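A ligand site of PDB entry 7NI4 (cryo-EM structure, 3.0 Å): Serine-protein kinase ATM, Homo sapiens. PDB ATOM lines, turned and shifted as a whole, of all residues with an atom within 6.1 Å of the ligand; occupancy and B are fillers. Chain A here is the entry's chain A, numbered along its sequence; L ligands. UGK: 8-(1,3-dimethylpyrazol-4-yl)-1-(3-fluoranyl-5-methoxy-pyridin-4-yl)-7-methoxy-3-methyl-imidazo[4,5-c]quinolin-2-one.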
ATOM      1  N   LEU A2692      -6.943 -27.649 -22.336  1.00  0.00           N
ATOM      2  CA  LEU A2692      -5.529 -27.935 -22.422  1.00  0.00           C
ATOM      3  C   LEU A2692      -5.116 -28.043 -23.882  1.00  0.00           C
ATOM      4  O   LEU A2692      -5.744 -28.763 -24.664  1.00  0.00           O
ATOM      5  CB  LEU A2692      -5.187 -29.227 -21.684  1.00  0.00           C
ATOM      6  CG  LEU A2692      -5.217 -29.157 -20.156  1.00  0.00           C
ATOM      7  CD1 LEU A2692      -5.111 -30.549 -19.560  1.00  0.00           C
ATOM      8  CD2 LEU A2692      -4.109 -28.265 -19.643  1.00  0.00           C
ATOM      9  N   ALA A2693      -4.058 -27.324 -24.251  1.00  0.00           N
ATOM     10  CA  ALA A2693      -3.548 -27.316 -25.627  1.00  0.00           C
ATOM     11  C   ALA A2693      -2.167 -27.942 -25.736  1.00  0.00           C
ATOM     12  O   ALA A2693      -1.464 -27.683 -26.719  1.00  0.00           O
ATOM     13  CB  ALA A2693      -3.531 -25.892 -26.170  1.00  0.00           C
ATOM     14  N   GLY A2694      -1.761 -28.750 -24.766  1.00  0.00           N
ATOM     15  CA  GLY A2694      -0.447 -29.365 -24.797  1.00  0.00           C
ATOM     16  C   GLY A2694       0.632 -28.464 -24.240  1.00  0.00           C
ATOM     17  O   GLY A2694       0.384 -27.345 -23.764  1.00  0.00           O
ATOM     18  N   GLY A2695       1.854 -28.964 -24.300  1.00  0.00           N
ATOM     19  CA  GLY A2695       3.017 -28.266 -23.793  1.00  0.00           C
ATOM     20  C   GLY A2695       3.863 -29.148 -22.891  1.00  0.00           C
ATOM     21  O   GLY A2695       3.503 -30.271 -22.534  1.00  0.00           O
ATOM     22  N   PRO A2699       0.293 -26.131 -19.823  1.00  0.00           N
ATOM     23  CA  PRO A2699      -0.359 -24.885 -19.407  1.00  0.00           C
ATOM     24  C   PRO A2699      -1.857 -24.967 -19.657  1.00  0.00           C
ATOM     25  O   PRO A2699      -2.324 -25.641 -20.585  1.00  0.00           O
ATOM     26  CB  PRO A2699       0.300 -23.826 -20.299  1.00  0.00           C
ATOM     27  CG  PRO A2699       0.815 -24.586 -21.470  1.00  0.00           C
ATOM     28  CD  PRO A2699       1.242 -25.912 -20.930  1.00  0.00           C
ATOM     29  N   ILE A2701      -5.756 -23.237 -20.227  1.00  0.00           N
ATOM     30  CA  ILE A2701      -6.459 -22.133 -20.864  1.00  0.00           C
ATOM     31  C   ILE A2701      -7.770 -21.925 -20.129  1.00  0.00           C
ATOM     32  O   ILE A2701      -8.540 -22.869 -19.926  1.00  0.00           O
ATOM     33  CB  ILE A2701      -6.713 -22.419 -22.358  1.00  0.00           C
ATOM     34  CG1 ILE A2701      -5.395 -22.560 -23.112  1.00  0.00           C
ATOM     35  CG2 ILE A2701      -7.550 -21.314 -22.975  1.00  0.00           C
ATOM     36  CD1 ILE A2701      -5.585 -23.096 -24.508  1.00  0.00           C
ATOM     37  N   LEU A2715      -4.088 -17.703 -20.919  1.00  0.00           N
ATOM     38  CA  LEU A2715      -3.191 -18.845 -20.762  1.00  0.00           C
ATOM     39  C   LEU A2715      -2.470 -18.727 -19.424  1.00  0.00           C
ATOM     40  O   LEU A2715      -1.675 -17.801 -19.227  1.00  0.00           O
ATOM     41  CB  LEU A2715      -2.191 -18.896 -21.913  1.00  0.00           C
ATOM     42  CG  LEU A2715      -1.218 -20.077 -21.914  1.00  0.00           C
ATOM     43  CD1 LEU A2715      -1.969 -21.391 -22.063  1.00  0.00           C
ATOM     44  CD2 LEU A2715      -0.214 -19.904 -23.037  1.00  0.00           C
ATOM     45  N   LYS A2717       0.169 -20.261 -16.922  1.00  0.00           N
ATOM     46  CA  LYS A2717       1.339 -21.134 -16.914  1.00  0.00           C
ATOM     47  C   LYS A2717       1.943 -21.180 -15.513  1.00  0.00           C
ATOM     48  O   LYS A2717       1.969 -20.183 -14.797  1.00  0.00           O
ATOM     49  CB  LYS A2717       2.400 -20.661 -17.910  1.00  0.00           C
ATOM     50  CG  LYS A2717       3.573 -21.615 -18.021  1.00  0.00           C
ATOM     51  CD  LYS A2717       4.640 -21.099 -18.947  1.00  0.00           C
ATOM     52  CE  LYS A2717       4.229 -21.202 -20.401  1.00  0.00           C
ATOM     53  NZ  LYS A2717       5.357 -20.796 -21.267  1.00  0.00           N
ATOM     54  N   ASP A2720       7.417 -21.827 -14.571  1.00  0.00           N
ATOM     55  CA  ASP A2720       8.197 -21.166 -15.596  1.00  0.00           C
ATOM     56  C   ASP A2720       8.253 -19.677 -15.308  1.00  0.00           C
ATOM     57  O   ASP A2720       7.275 -19.083 -14.841  1.00  0.00           O
ATOM     58  CB  ASP A2720       7.609 -21.410 -16.995  1.00  0.00           C
ATOM     59  CG  ASP A2720       8.554 -21.011 -18.106  1.00  0.00           C
ATOM     60  OD1 ASP A2720       9.680 -20.552 -17.803  1.00  0.00           O
ATOM     61  OD2 ASP A2720       8.167 -21.144 -19.290  1.00  0.00           O
ATOM     62  N   LEU A2722       8.224 -15.955 -16.416  1.00  0.00           N
ATOM     63  CA  LEU A2722       7.634 -15.205 -17.506  1.00  0.00           C
ATOM     64  C   LEU A2722       8.044 -13.744 -17.539  1.00  0.00           C
ATOM     65  O   LEU A2722       7.535 -12.984 -18.369  1.00  0.00           O
ATOM     66  CB  LEU A2722       6.105 -15.308 -17.453  1.00  0.00           C
ATOM     67  CG  LEU A2722       5.499 -16.688 -17.724  1.00  0.00           C
ATOM     68  CD1 LEU A2722       4.066 -16.545 -18.224  1.00  0.00           C
ATOM     69  CD2 LEU A2722       6.346 -17.469 -18.716  1.00  0.00           C
ATOM     70  N   ASP A2725       9.690 -12.791 -20.918  1.00  0.00           N
ATOM     71  CA  ASP A2725       8.726 -12.571 -21.992  1.00  0.00           C
ATOM     72  C   ASP A2725       8.105 -11.184 -21.904  1.00  0.00           C
ATOM     73  O   ASP A2725       7.965 -10.506 -22.917  1.00  0.00           O
ATOM     74  CB  ASP A2725       7.645 -13.655 -21.950  1.00  0.00           C
ATOM     75  CG  ASP A2725       8.165 -15.026 -22.326  1.00  0.00           C
ATOM     76  OD1 ASP A2725       9.131 -15.089 -23.117  1.00  0.00           O
ATOM     77  OD2 ASP A2725       7.619 -16.020 -21.831  1.00  0.00           O
ATOM     78  N   TYR A2755       1.886  -9.420 -27.585  1.00  0.00           N
ATOM     79  CA  TYR A2755       0.894  -9.857 -26.606  1.00  0.00           C
ATOM     80  C   TYR A2755       1.379  -9.429 -25.232  1.00  0.00           C
ATOM     81  O   TYR A2755       2.572  -9.221 -25.008  1.00  0.00           O
ATOM     82  CB  TYR A2755       0.679 -11.370 -26.652  1.00  0.00           C
ATOM     83  CG  TYR A2755       1.960 -12.160 -26.670  1.00  0.00           C
ATOM     84  CD1 TYR A2755       2.564 -12.565 -25.482  1.00  0.00           C
ATOM     85  CD2 TYR A2755       2.582 -12.497 -27.862  1.00  0.00           C
ATOM     86  CE1 TYR A2755       3.739 -13.282 -25.495  1.00  0.00           C
ATOM     87  CE2 TYR A2755       3.757 -13.214 -27.874  1.00  0.00           C
ATOM     88  CZ  TYR A2755       4.330 -13.605 -26.687  1.00  0.00           C
ATOM     89  OH  TYR A2755       5.509 -14.326 -26.692  1.00  0.00           O
ATOM     90  N   LYS A2756       0.437  -9.280 -24.296  1.00  0.00           N
ATOM     91  CA  LYS A2756       0.773  -8.883 -22.936  1.00  0.00           C
ATOM     92  C   LYS A2756       0.968 -10.098 -22.057  1.00  0.00           C
ATOM     93  O   LYS A2756       0.123 -11.010 -22.047  1.00  0.00           O
ATOM     94  CB  LYS A2756      -0.294  -7.971 -22.331  1.00  0.00           C
ATOM     95  CG  LYS A2756       0.102  -7.462 -20.955  1.00  0.00           C
ATOM     96  CD  LYS A2756      -0.965  -6.600 -20.315  1.00  0.00           C
ATOM     97  CE  LYS A2756      -1.629  -5.693 -21.323  1.00  0.00           C
ATOM     98  NZ  LYS A2756      -2.248  -4.509 -20.659  1.00  0.00           N
ATOM     99  N   VAL A2757       2.069 -10.119 -21.322  1.00  0.00           N
ATOM    100  CA  VAL A2757       2.381 -11.164 -20.353  1.00  0.00           C
ATOM    101  C   VAL A2757       2.334 -10.537 -18.972  1.00  0.00           C
ATOM    102  O   VAL A2757       2.963  -9.498 -18.731  1.00  0.00           O
ATOM    103  CB  VAL A2757       3.755 -11.801 -20.613  1.00  0.00           C
ATOM    104  CG1 VAL A2757       4.084 -12.804 -19.532  1.00  0.00           C
ATOM    105  CG2 VAL A2757       3.775 -12.459 -21.983  1.00  0.00           C
ATOM    106  N   LEU A2767      -0.724 -14.980 -19.301  1.00  0.00           N
ATOM    107  CA  LEU A2767      -0.450 -14.237 -20.519  1.00  0.00           C
ATOM    108  C   LEU A2767      -1.590 -14.433 -21.509  1.00  0.00           C
ATOM    109  O   LEU A2767      -2.327 -15.411 -21.440  1.00  0.00           O
ATOM    110  CB  LEU A2767       0.890 -14.673 -21.152  1.00  0.00           C
ATOM    111  CG  LEU A2767       1.090 -16.119 -21.588  1.00  0.00           C
ATOM    112  CD1 LEU A2767       2.278 -16.193 -22.537  1.00  0.00           C
ATOM    113  CD2 LEU A2767       1.325 -17.029 -20.397  1.00  0.00           C
ATOM    114  N   GLU A2768      -1.697 -13.466 -22.425  1.00  0.00           N
ATOM    115  CA  GLU A2768      -2.818 -13.458 -23.368  1.00  0.00           C
ATOM    116  C   GLU A2768      -2.721 -14.627 -24.338  1.00  0.00           C
ATOM    117  O   GLU A2768      -1.635 -14.970 -24.816  1.00  0.00           O
ATOM    118  CB  GLU A2768      -2.821 -12.144 -24.145  1.00  0.00           C
ATOM    119  CG  GLU A2768      -3.874 -12.070 -25.237  1.00  0.00           C
ATOM    120  CD  GLU A2768      -3.799 -10.781 -26.030  1.00  0.00           C
ATOM    121  OE1 GLU A2768      -3.046  -9.874 -25.611  1.00  0.00           O
ATOM    122  OE2 GLU A2768      -4.497 -10.668 -27.050  1.00  0.00           O
ATOM    123  N   TRP A2769      -3.868 -15.252 -24.617  1.00  0.00           N
ATOM    124  CA  TRP A2769      -3.953 -16.322 -25.602  1.00  0.00           C
ATOM    125  C   TRP A2769      -4.357 -15.733 -26.947  1.00  0.00           C
ATOM    126  O   TRP A2769      -5.385 -15.066 -27.060  1.00  0.00           O
ATOM    127  CB  TRP A2769      -4.983 -17.366 -25.156  1.00  0.00           C
ATOM    128  CG  TRP A2769      -5.251 -18.444 -26.150  1.00  0.00           C
ATOM    129  CD1 TRP A2769      -6.240 -18.480 -27.072  1.00  0.00           C
ATOM    130  CD2 TRP A2769      -4.513 -19.671 -26.315  1.00  0.00           C
ATOM    131  NE1 TRP A2769      -6.174 -19.635 -27.807  1.00  0.00           N
ATOM    132  CE2 TRP A2769      -5.113 -20.387 -27.358  1.00  0.00           C
ATOM    133  CE3 TRP A2769      -3.398 -20.219 -25.675  1.00  0.00           C
ATOM    134  CZ2 TRP A2769      -4.653 -21.621 -27.780  1.00  0.00           C
ATOM    135  CZ3 TRP A2769      -2.938 -21.453 -26.097  1.00  0.00           C
ATOM    136  CH2 TRP A2769      -3.563 -22.142 -27.138  1.00  0.00           C
ATOM    137  N   CYS A2770      -3.531 -15.982 -27.962  1.00  0.00           N
ATOM    138  CA  CYS A2770      -3.770 -15.435 -29.290  1.00  0.00           C
ATOM    139  C   CYS A2770      -4.817 -16.292 -30.002  1.00  0.00           C
ATOM    140  O   CYS A2770      -4.560 -17.449 -30.329  1.00  0.00           O
ATOM    141  CB  CYS A2770      -2.474 -15.383 -30.093  1.00  0.00           C
ATOM    142  SG  CYS A2770      -1.280 -14.159 -29.500  1.00  0.00           S
ATOM    143  N   THR A2771      -5.984 -15.708 -30.249  1.00  0.00           N
ATOM    144  CA  THR A2771      -7.057 -16.428 -30.914  1.00  0.00           C
ATOM    145  C   THR A2771      -6.853 -16.426 -32.420  1.00  0.00           C
ATOM    146  O   THR A2771      -6.329 -15.471 -32.998  1.00  0.00           O
ATOM    147  CB  THR A2771      -8.412 -15.814 -30.577  1.00  0.00           C
ATOM    148  OG1 THR A2771      -8.451 -14.461 -31.029  1.00  0.00           O
ATOM    149  CG2 THR A2771      -8.648 -15.843 -29.068  1.00  0.00           C
ATOM    150  N   THR A2773      -4.871 -18.413 -34.143  1.00  0.00           N
ATOM    151  CA  THR A2773      -3.494 -18.713 -34.515  1.00  0.00           C
ATOM    152  C   THR A2773      -3.239 -20.211 -34.397  1.00  0.00           C
ATOM    153  O   THR A2773      -3.912 -20.903 -33.617  1.00  0.00           O
ATOM    154  CB  THR A2773      -2.508 -17.948 -33.632  1.00  0.00           C
ATOM    155  OG1 THR A2773      -2.649 -18.375 -32.269  1.00  0.00           O
ATOM    156  CG2 THR A2773      -2.762 -16.460 -33.718  1.00  0.00           C
ATOM    157  N   VAL A2774      -2.296 -20.709 -35.181  1.00  0.00           N
ATOM    158  CA  VAL A2774      -1.898 -22.111 -35.125  1.00  0.00           C
ATOM    159  C   VAL A2774      -0.372 -22.178 -35.228  1.00  0.00           C
ATOM    160  O   VAL A2774       0.224 -21.389 -35.968  1.00  0.00           O
ATOM    161  CB  VAL A2774      -2.587 -22.924 -36.223  1.00  0.00           C
ATOM    162  CG1 VAL A2774      -2.181 -22.438 -37.605  1.00  0.00           C
ATOM    163  CG2 VAL A2774      -2.295 -24.409 -36.068  1.00  0.00           C
ATOM    164  N   PRO A2775       0.287 -23.059 -34.477  1.00  0.00           N
ATOM    165  CA  PRO A2775       1.734 -23.229 -34.655  1.00  0.00           C
ATOM    166  C   PRO A2775       2.060 -23.678 -36.075  1.00  0.00           C
ATOM    167  O   PRO A2775       1.343 -24.491 -36.662  1.00  0.00           O
ATOM    168  CB  PRO A2775       2.096 -24.298 -33.626  1.00  0.00           C
ATOM    169  CG  PRO A2775       1.055 -24.179 -32.593  1.00  0.00           C
ATOM    170  CD  PRO A2775      -0.209 -23.827 -33.319  1.00  0.00           C
ATOM    171  N   GLN A2874       7.689 -24.879 -33.008  1.00  0.00           N
ATOM    172  CA  GLN A2874       6.633 -24.685 -32.015  1.00  0.00           C
ATOM    173  C   GLN A2874       6.658 -23.293 -31.389  1.00  0.00           C
ATOM    174  O   GLN A2874       5.718 -22.940 -30.670  1.00  0.00           O
ATOM    175  CB  GLN A2874       6.727 -25.749 -30.931  1.00  0.00           C
ATOM    176  CG  GLN A2874       6.705 -27.169 -31.462  1.00  0.00           C
ATOM    177  CD  GLN A2874       5.345 -27.570 -31.986  1.00  0.00           C
ATOM    178  OE1 GLN A2874       4.328 -27.046 -31.547  1.00  0.00           O
ATOM    179  NE2 GLN A2874       5.328 -28.508 -32.925  1.00  0.00           N
ATOM    180  N   ASN A2875       7.702 -22.514 -31.633  1.00  0.00           N
ATOM    181  CA  ASN A2875       7.809 -21.182 -31.043  1.00  0.00           C
ATOM    182  C   ASN A2875       7.286 -20.080 -31.948  1.00  0.00           C
ATOM    183  O   ASN A2875       7.374 -18.907 -31.593  1.00  0.00           O
ATOM    184  CB  ASN A2875       9.269 -20.890 -30.677  1.00  0.00           C
ATOM    185  CG  ASN A2875       9.674 -21.518 -29.366  1.00  0.00           C
ATOM    186  OD1 ASN A2875       8.850 -22.116 -28.669  1.00  0.00           O
ATOM    187  ND2 ASN A2875      10.943 -21.398 -29.016  1.00  0.00           N
ATOM    188  N   ILE A2876       6.750 -20.428 -33.118  1.00  0.00           N
ATOM    189  CA  ILE A2876       6.197 -19.458 -34.050  1.00  0.00           C
ATOM    190  C   ILE A2876       4.766 -19.848 -34.371  1.00  0.00           C
ATOM    191  O   ILE A2876       4.488 -21.012 -34.673  1.00  0.00           O
ATOM    192  CB  ILE A2876       7.032 -19.368 -35.340  1.00  0.00           C
ATOM    193  CG1 ILE A2876       8.526 -19.289 -35.015  1.00  0.00           C
ATOM    194  CG2 ILE A2876       6.609 -18.158 -36.165  1.00  0.00           C
ATOM    195  CD1 ILE A2876       9.416 -19.294 -36.234  1.00  0.00           C
ATOM    196  N   LEU A2877       3.863 -18.880 -34.305  1.00  0.00           N
ATOM    197  CA  LEU A2877       2.460 -19.079 -34.665  1.00  0.00           C
ATOM    198  C   LEU A2877       2.114 -18.199 -35.851  1.00  0.00           C
ATOM    199  O   LEU A2877       2.694 -17.130 -36.039  1.00  0.00           O
ATOM    200  CB  LEU A2877       1.522 -18.748 -33.500  1.00  0.00           C
ATOM    201  CG  LEU A2877       1.963 -19.161 -32.095  1.00  0.00           C
ATOM    202  CD1 LEU A2877       0.966 -18.655 -31.081  1.00  0.00           C
ATOM    203  CD2 LEU A2877       2.101 -20.651 -32.012  1.00  0.00           C
ATOM    204  N   ILE A2888       6.848 -16.556 -29.897  1.00  0.00           N
ATOM    205  CA  ILE A2888       6.604 -16.834 -28.490  1.00  0.00           C
ATOM    206  C   ILE A2888       7.841 -17.534 -27.918  1.00  0.00           C
ATOM    207  O   ILE A2888       8.752 -17.921 -28.639  1.00  0.00           O
ATOM    208  CB  ILE A2888       5.355 -17.696 -28.269  1.00  0.00           C
ATOM    209  CG1 ILE A2888       5.511 -19.057 -28.936  1.00  0.00           C
ATOM    210  CG2 ILE A2888       4.118 -16.981 -28.809  1.00  0.00           C
ATOM    211  CD1 ILE A2888       4.375 -20.001 -28.668  1.00  0.00           C
ATOM    212  N   ASP A2889       7.848 -17.667 -26.589  1.00  0.00           N
ATOM    213  CA  ASP A2889       8.942 -18.306 -25.850  1.00  0.00           C
ATOM    214  C   ASP A2889      10.246 -17.562 -26.148  1.00  0.00           C
ATOM    215  O   ASP A2889      11.152 -18.053 -26.834  1.00  0.00           O
ATOM    216  CB  ASP A2889       8.998 -19.804 -26.176  1.00  0.00           C
ATOM    217  CG  ASP A2889      10.230 -20.525 -25.576  1.00  0.00           C
ATOM    218  OD1 ASP A2889      11.168 -19.896 -25.050  1.00  0.00           O
ATOM    219  OD2 ASP A2889      10.238 -21.774 -25.648  1.00  0.00           O
ATOM    220  N   LEU A2890      10.286 -16.310 -25.677  1.00  0.00           N
ATOM    221  CA  LEU A2890      11.382 -15.397 -25.940  1.00  0.00           C
ATOM    222  C   LEU A2890      12.494 -15.499 -24.905  1.00  0.00           C
ATOM    223  O   LEU A2890      13.178 -14.503 -24.628  1.00  0.00           O
ATOM    224  CB  LEU A2890      10.859 -13.963 -26.014  1.00  0.00           C
ATOM    225  CG  LEU A2890       9.876 -13.664 -27.137  1.00  0.00           C
ATOM    226  CD1 LEU A2890       9.310 -12.265 -26.984  1.00  0.00           C
ATOM    227  CD2 LEU A2890      10.537 -13.821 -28.490  1.00  0.00           C
HETATM  228  C1  UGK L   1      -0.759 -24.248 -24.971  1.00  0.00           C
HETATM  229  N6  UGK L   1       2.975 -24.606 -26.787  1.00  0.00           N
HETATM  230  C7  UGK L   1       1.753 -24.546 -26.249  1.00  0.00           C
HETATM  231  C8  UGK L   1       0.699 -23.866 -26.826  1.00  0.00           C
HETATM  232  C9  UGK L   1       0.896 -23.217 -28.041  1.00  0.00           C
HETATM  233  C11 UGK L   1      -2.977 -22.298 -30.970  1.00  0.00           C
HETATM  234  C13 UGK L   1      -1.030 -23.112 -29.621  1.00  0.00           C
HETATM  235  C15 UGK L   1       1.139 -15.636 -25.764  1.00  0.00           C
HETATM  236  C19 UGK L   1       3.752 -18.491 -24.893  1.00  0.00           C
HETATM  237  C22 UGK L   1       3.125 -20.569 -24.475  1.00  0.00           C
HETATM  238  C24 UGK L   1       1.154 -20.285 -26.856  1.00  0.00           C
HETATM  239  C27 UGK L   1      -0.106 -17.801 -27.056  1.00  0.00           C
HETATM  240  C30 UGK L   1      -0.499 -21.182 -28.542  1.00  0.00           C
HETATM  241  C31 UGK L   1      -1.578 -20.932 -29.355  1.00  0.00           C
HETATM  242  C32 UGK L   1      -2.124 -19.648 -29.372  1.00  0.00           C
HETATM  243  C17 UGK L   1       2.421 -21.881 -24.423  1.00  0.00           C
HETATM  244  C18 UGK L   1       5.792 -18.540 -23.441  1.00  0.00           C
HETATM  245  C23 UGK L   1       2.770 -19.401 -25.207  1.00  0.00           C
HETATM  246  C25 UGK L   1       1.611 -19.216 -26.113  1.00  0.00           C
HETATM  247  C26 UGK L   1       0.963 -17.979 -26.225  1.00  0.00           C
HETATM  248  C28 UGK L   1      -0.587 -18.882 -27.831  1.00  0.00           C
HETATM  249  C29 UGK L   1       0.050 -20.144 -27.726  1.00  0.00           C
HETATM  250  C4  UGK L   1       2.182 -23.290 -28.581  1.00  0.00           C
HETATM  251  C5  UGK L   1       3.186 -23.979 -27.945  1.00  0.00           C
HETATM  252  F3  UGK L   1       2.441 -22.673 -29.757  1.00  0.00           F
HETATM  253  N12 UGK L   1      -1.898 -22.112 -30.016  1.00  0.00           N
HETATM  254  N14 UGK L   1      -0.165 -22.518 -28.703  1.00  0.00           N
HETATM  255  N20 UGK L   1       4.588 -19.101 -24.055  1.00  0.00           N
HETATM  256  N21 UGK L   1       4.234 -20.376 -23.768  1.00  0.00           N
HETATM  257  N33 UGK L   1      -1.669 -18.652 -28.653  1.00  0.00           N
HETATM  258  O10 UGK L   1      -1.031 -24.264 -29.997  1.00  0.00           O
HETATM  259  O16 UGK L   1       1.491 -16.986 -25.446  1.00  0.00           O
HETATM  260  O2  UGK L   1      -0.560 -23.790 -26.311  1.00  0.00           O
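NZ of Lys 2717 lies within salt-bridge range of OD2 of Asp 2720 (3.5 Å).
The backbone carbonyl oxygen (O) of Lys 2756 is in hydrogen-bond range of the backbone NH (N) of Glu 2768, at 3.1 Å.
The backbone carbonyl oxygen (O) of Leu 2767 sits at hydrogen-bond distance from the backbone NH (N) of Leu 2715.
OG1 of Thr 2773 sits at hydrogen-bond distance from O of Cys 2770, 2.9 Å away.
N of Ile 2888 is in hydrogen-bond range of O of Asn 2875, at 2.9 Å.
The backbone NH (N) of Leu 2890 lies within hydrogen-bond range of the side-chain carboxylate (OD1) of Asp 2725, 3.1 Å away.
OD2 of Asp 2889 sits close to OD1 of Asn 2875, at 3.3 Å.
A fluorine (F3) of the ligand lies close to the backbone carbonyl oxygen (O) of Gln 2874 (3.4 Å).
Ala 2693 touches the ligand.
Gly 2694 touches the ligand.
Pro 2699 touches the ligand.
Leu 2715 touches the ligand (CD2 to C17, 3.6 Å).
Asp 2725 touches the ligand (OD2 to C18, 3.5 Å).
Tyr 2755 touches the ligand.
Leu 2767 touches the ligand (CD1 to O16, 3.1 Å).
O of Glu 2768 touches C15 of the ligand, at 3.0 Å.
Trp 2769 touches the ligand.
Thr 2773 touches the ligand.
Pro 2775 touches the ligand.
Leu 2877 touches the ligand (CD2 to F3, 3.0 Å).
Ile 2888 touches the ligand (CD1 to F3, 3.5 Å).
N of Asp 2889 touches C18 of the ligand, 3.9 Å away.
17 residues have an atom within 4 Å of the ligand: Ala 2693, Gly 2694, Pro 2699, Leu 2715, Lys 2717, Asp 2725, Tyr 2755, Leu 2767, Glu 2768, Trp 2769, Cys 2770, Thr 2773, Pro 2775, Gln 2874, Leu 2877, Ile 2888 and Asp 2889.
NZ of Lys 2717 is in hydrogen-bond range of N21 of the ligand, at 2.8 Å.
A nitrogen (N33) of the ligand sits at hydrogen-bond distance from the backbone NH (N) of Cys 2770, 3.3 Å away.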
